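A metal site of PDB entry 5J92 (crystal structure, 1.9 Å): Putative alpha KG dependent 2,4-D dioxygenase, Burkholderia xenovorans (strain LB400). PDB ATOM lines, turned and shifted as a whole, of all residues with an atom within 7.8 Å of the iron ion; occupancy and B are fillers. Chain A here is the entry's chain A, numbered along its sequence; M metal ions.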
ATOM      1  N   ASN A 114      -2.934  14.426   8.285  1.00  0.00           N
ATOM      2  CA  ASN A 114      -2.745  13.358   9.261  1.00  0.00           C
ATOM      3  C   ASN A 114      -4.025  13.075  10.022  1.00  0.00           C
ATOM      4  O   ASN A 114      -4.334  11.924  10.315  1.00  0.00           O
ATOM      5  CB  ASN A 114      -1.622  13.722  10.221  1.00  0.00           C
ATOM      6  CG  ASN A 114      -0.292  13.804   9.533  1.00  0.00           C
ATOM      7  OD1 ASN A 114      -0.115  13.256   8.438  1.00  0.00           O
ATOM      8  ND2 ASN A 114       0.652  14.519  10.146  1.00  0.00           N
ATOM      9  N   THR A 117      -6.336  11.019   7.481  1.00  0.00           N
ATOM     10  CA  THR A 117      -5.846   9.690   7.130  1.00  0.00           C
ATOM     11  C   THR A 117      -5.795   8.767   8.341  1.00  0.00           C
ATOM     12  O   THR A 117      -5.933   7.553   8.184  1.00  0.00           O
ATOM     13  CB  THR A 117      -4.466   9.771   6.483  1.00  0.00           C
ATOM     14  OG1 THR A 117      -3.527  10.300   7.426  1.00  0.00           O
ATOM     15  CG2 THR A 117      -4.527  10.679   5.259  1.00  0.00           C
ATOM     16  N   SER A 118      -5.640   9.326   9.539  1.00  0.00           N
ATOM     17  CA  SER A 118      -5.636   8.493  10.740  1.00  0.00           C
ATOM     18  C   SER A 118      -7.023   7.973  11.100  1.00  0.00           C
ATOM     19  O   SER A 118      -7.128   7.100  11.976  1.00  0.00           O
ATOM     20  CB  SER A 118      -5.054   9.272  11.930  1.00  0.00           C
ATOM     21  OG  SER A 118      -3.644   9.291  11.860  1.00  0.00           O
ATOM     22  N   ARG A 120      -8.644   6.203   9.059  1.00  0.00           N
ATOM     23  CA  ARG A 120      -8.650   4.931   8.360  1.00  0.00           C
ATOM     24  C   ARG A 120      -7.730   3.940   9.088  1.00  0.00           C
ATOM     25  O   ARG A 120      -6.655   4.319   9.573  1.00  0.00           O
ATOM     26  CB  ARG A 120      -8.200   5.131   6.893  1.00  0.00           C
ATOM     27  CG  ARG A 120      -9.240   5.929   6.073  1.00  0.00           C
ATOM     28  CD  ARG A 120      -8.632   6.854   5.032  1.00  0.00           C
ATOM     29  NE  ARG A 120      -9.656   7.531   4.228  1.00  0.00           N
ATOM     30  CZ  ARG A 120     -10.192   8.728   4.506  1.00  0.00           C
ATOM     31  NH1 ARG A 120      -9.810   9.398   5.585  1.00  0.00           N
ATOM     32  NH2 ARG A 120     -11.098   9.263   3.703  1.00  0.00           N
ATOM     33  N   HIS A 122      -4.961   1.584  10.093  1.00  0.00           N
ATOM     34  CA  HIS A 122      -3.599   1.475   9.583  1.00  0.00           C
ATOM     35  C   HIS A 122      -2.679   0.964  10.687  1.00  0.00           C
ATOM     36  O   HIS A 122      -3.046   0.919  11.864  1.00  0.00           O
ATOM     37  CB  HIS A 122      -3.136   2.829   9.036  1.00  0.00           C
ATOM     38  CG  HIS A 122      -3.081   3.897  10.076  1.00  0.00           C
ATOM     39  ND1 HIS A 122      -4.223   4.449  10.625  1.00  0.00           N
ATOM     40  CD2 HIS A 122      -2.029   4.488  10.692  1.00  0.00           C
ATOM     41  CE1 HIS A 122      -3.873   5.343  11.541  1.00  0.00           C
ATOM     42  NE2 HIS A 122      -2.553   5.387  11.593  1.00  0.00           N
ATOM     43  N   SER A 123      -1.474   0.554  10.286  1.00  0.00           N
ATOM     44  CA  SER A 123      -0.384   0.224  11.197  1.00  0.00           C
ATOM     45  C   SER A 123       0.763   1.197  10.932  1.00  0.00           C
ATOM     46  O   SER A 123       1.137   1.405   9.771  1.00  0.00           O
ATOM     47  CB  SER A 123       0.092  -1.226  10.993  1.00  0.00           C
ATOM     48  OG  SER A 123       1.108  -1.565  11.920  1.00  0.00           O
ATOM     49  N   ASP A 124       1.278   1.818  11.989  1.00  0.00           N
ATOM     50  CA  ASP A 124       2.179   2.969  11.852  1.00  0.00           C
ATOM     51  C   ASP A 124       3.417   2.649  11.018  1.00  0.00           C
ATOM     52  O   ASP A 124       4.142   1.690  11.296  1.00  0.00           O
ATOM     53  CB  ASP A 124       2.610   3.476  13.229  1.00  0.00           C
ATOM     54  CG  ASP A 124       1.514   4.270  13.888  1.00  0.00           C
ATOM     55  OD1 ASP A 124       0.500   4.487  13.190  1.00  0.00           O
ATOM     56  OD2 ASP A 124       1.653   4.671  15.080  1.00  0.00           O
ATOM     57  N   ALA A 125       3.680   3.512  10.029  1.00  0.00           N
ATOM     58  CA  ALA A 125       4.877   3.458   9.194  1.00  0.00           C
ATOM     59  C   ALA A 125       5.051   2.115   8.477  1.00  0.00           C
ATOM     60  O   ALA A 125       6.173   1.750   8.087  1.00  0.00           O
ATOM     61  CB  ALA A 125       6.143   3.796   9.999  1.00  0.00           C
ATOM     62  N   SER A 135       4.005   2.458  19.408  1.00  0.00           N
ATOM     63  CA  SER A 135       3.624   3.854  19.382  1.00  0.00           C
ATOM     64  C   SER A 135       3.070   4.244  20.750  1.00  0.00           C
ATOM     65  O   SER A 135       2.544   3.397  21.478  1.00  0.00           O
ATOM     66  CB  SER A 135       2.582   4.121  18.286  1.00  0.00           C
ATOM     67  OG  SER A 135       3.132   3.903  16.993  1.00  0.00           O
ATOM     68  N   LEU A 137       0.921   7.423  22.968  1.00  0.00           N
ATOM     69  CA  LEU A 137       0.041   8.585  22.929  1.00  0.00           C
ATOM     70  C   LEU A 137      -0.304   8.969  24.361  1.00  0.00           C
ATOM     71  O   LEU A 137      -0.846   8.156  25.107  1.00  0.00           O
ATOM     72  CB  LEU A 137      -1.256   8.295  22.152  1.00  0.00           C
ATOM     73  CG  LEU A 137      -1.394   8.627  20.676  1.00  0.00           C
ATOM     74  CD1 LEU A 137      -2.808   8.278  20.177  1.00  0.00           C
ATOM     75  CD2 LEU A 137      -1.061  10.092  20.390  1.00  0.00           C
ATOM     76  N   THR A 149      -9.687   6.141  20.338  1.00  0.00           N
ATOM     77  CA  THR A 149      -8.749   5.410  19.497  1.00  0.00           C
ATOM     78  C   THR A 149      -9.170   3.952  19.541  1.00  0.00           C
ATOM     79  O   THR A 149      -9.420   3.408  20.620  1.00  0.00           O
ATOM     80  CB  THR A 149      -7.294   5.578  19.962  1.00  0.00           C
ATOM     81  OG1 THR A 149      -6.980   6.952  20.091  1.00  0.00           O
ATOM     82  CG2 THR A 149      -6.340   4.976  18.917  1.00  0.00           C
ATOM     83  N   HIS A 222      -2.142   1.403   4.201  1.00  0.00           N
ATOM     84  CA  HIS A 222      -1.004   1.621   3.333  1.00  0.00           C
ATOM     85  C   HIS A 222      -0.799   0.496   2.338  1.00  0.00           C
ATOM     86  O   HIS A 222      -0.146   0.717   1.313  1.00  0.00           O
ATOM     87  CB  HIS A 222       0.267   1.807   4.171  1.00  0.00           C
ATOM     88  CG  HIS A 222       0.136   2.835   5.250  1.00  0.00           C
ATOM     89  ND1 HIS A 222       0.438   2.582   6.570  1.00  0.00           N
ATOM     90  CD2 HIS A 222      -0.284   4.119   5.201  1.00  0.00           C
ATOM     91  CE1 HIS A 222       0.223   3.670   7.284  1.00  0.00           C
ATOM     92  NE2 HIS A 222      -0.218   4.618   6.483  1.00  0.00           N
ATOM     93  N   TRP A 264       0.985   1.007  22.192  1.00  0.00           N
ATOM     94  CA  TRP A 264       0.469  -0.100  21.394  1.00  0.00           C
ATOM     95  C   TRP A 264       1.512  -0.628  20.433  1.00  0.00           C
ATOM     96  O   TRP A 264       2.375   0.111  19.942  1.00  0.00           O
ATOM     97  CB  TRP A 264      -0.842   0.279  20.653  1.00  0.00           C
ATOM     98  CG  TRP A 264      -0.717   1.227  19.478  1.00  0.00           C
ATOM     99  CD1 TRP A 264      -0.490   0.912  18.159  1.00  0.00           C
ATOM    100  CD2 TRP A 264      -0.851   2.650  19.515  1.00  0.00           C
ATOM    101  NE1 TRP A 264      -0.452   2.058  17.381  1.00  0.00           N
ATOM    102  CE2 TRP A 264      -0.675   3.138  18.198  1.00  0.00           C
ATOM    103  CE3 TRP A 264      -1.085   3.568  20.549  1.00  0.00           C
ATOM    104  CZ2 TRP A 264      -0.749   4.480  17.889  1.00  0.00           C
ATOM    105  CZ3 TRP A 264      -1.154   4.914  20.232  1.00  0.00           C
ATOM    106  CH2 TRP A 264      -0.974   5.357  18.920  1.00  0.00           C
ATOM    107  N   ASN A 266       2.447  -1.954  17.073  1.00  0.00           N
ATOM    108  CA  ASN A 266       2.023  -1.956  15.681  1.00  0.00           C
ATOM    109  C   ASN A 266       2.268  -3.297  14.992  1.00  0.00           C
ATOM    110  O   ASN A 266       1.674  -3.558  13.943  1.00  0.00           O
ATOM    111  CB  ASN A 266       2.740  -0.835  14.924  1.00  0.00           C
ATOM    112  CG  ASN A 266       2.309   0.546  15.393  1.00  0.00           C
ATOM    113  OD1 ASN A 266       1.249   1.018  15.005  1.00  0.00           O
ATOM    114  ND2 ASN A 266       3.117   1.176  16.236  1.00  0.00           N
ATOM    115  N   HIS A 271      -4.892   0.409  13.978  1.00  0.00           N
ATOM    116  CA  HIS A 271      -5.616   1.326  14.849  1.00  0.00           C
ATOM    117  C   HIS A 271      -6.163   2.464  14.001  1.00  0.00           C
ATOM    118  O   HIS A 271      -5.749   2.669  12.860  1.00  0.00           O
ATOM    119  CB  HIS A 271      -4.722   1.876  15.962  1.00  0.00           C
ATOM    120  CG  HIS A 271      -3.674   2.804  15.449  1.00  0.00           C
ATOM    121  ND1 HIS A 271      -2.516   2.360  14.848  1.00  0.00           N
ATOM    122  CD2 HIS A 271      -3.628   4.152  15.418  1.00  0.00           C
ATOM    123  CE1 HIS A 271      -1.796   3.396  14.472  1.00  0.00           C
ATOM    124  NE2 HIS A 271      -2.445   4.498  14.817  1.00  0.00           N
ATOM    125  N   ARG A 272      -7.077   3.221  14.584  1.00  0.00           N
ATOM    126  CA  ARG A 272      -7.608   4.390  13.907  1.00  0.00           C
ATOM    127  C   ARG A 272      -8.156   5.337  14.950  1.00  0.00           C
ATOM    128  O   ARG A 272      -8.571   4.899  16.022  1.00  0.00           O
ATOM    129  CB  ARG A 272      -8.713   4.008  12.900  1.00  0.00           C
ATOM    130  CG  ARG A 272     -10.011   3.542  13.567  1.00  0.00           C
ATOM    131  CD  ARG A 272     -11.110   3.200  12.545  1.00  0.00           C
ATOM    132  NE  ARG A 272     -12.352   2.819  13.246  1.00  0.00           N
ATOM    133  CZ  ARG A 272     -13.544   2.725  12.652  1.00  0.00           C
ATOM    134  NH1 ARG A 272     -13.648   2.993  11.363  1.00  0.00           N
ATOM    135  NH2 ARG A 272     -14.626   2.399  13.355  1.00  0.00           N
ATOM    136  N   GLY A 273      -8.170   6.625  14.613  1.00  0.00           N
ATOM    137  CA  GLY A 273      -8.827   7.609  15.442  1.00  0.00           C
ATOM    138  C   GLY A 273     -10.268   7.829  14.986  1.00  0.00           C
ATOM    139  O   GLY A 273     -10.608   7.598  13.833  1.00  0.00           O
ATOM    140  N   THR A 289       7.194   7.582  18.876  1.00  0.00           N
ATOM    141  CA  THR A 289       7.177   6.363  18.071  1.00  0.00           C
ATOM    142  C   THR A 289       8.557   5.717  18.092  1.00  0.00           C
ATOM    143  O   THR A 289       9.573   6.399  17.980  1.00  0.00           O
ATOM    144  CB  THR A 289       6.734   6.657  16.631  1.00  0.00           C
ATOM    145  OG1 THR A 289       5.498   7.389  16.668  1.00  0.00           O
ATOM    146  CG2 THR A 289       6.514   5.355  15.861  1.00  0.00           C
HETATM  147 FE    FE M   1      -1.237   6.179  13.516  1.00  0.00          FE
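The iron ion is bound by a ring nitrogen (NE2) of His 271 (2.4 Å). OD1 of Asp 124 binds the iron ion (2.4 Å). A ring nitrogen (NE2) of His 122 is bound to the iron ion (2.5 Å).
The indole nitrogen (NE1) of Trp 264 is in hydrogen-bond range of a ring nitrogen (ND1) of His 271, at 3.3 Å. N of Asp 124 is in hydrogen-bond range of OD1 of Asn 266, 3.1 Å away. OG of Ser 135 is in hydrogen-bond range of OD2 of Asp 124, at 2.5 Å. A ring nitrogen (ND1) of His 122 is in hydrogen-bond range of the backbone carbonyl oxygen (O) of Arg 120, 2.7 Å away.
Three residues have an atom within 4 Å of the iron ion: His 122, Asp 124 and His 271. The nearest printed residue that does not touch the iron ion is Ser 118 (4.3 Å).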
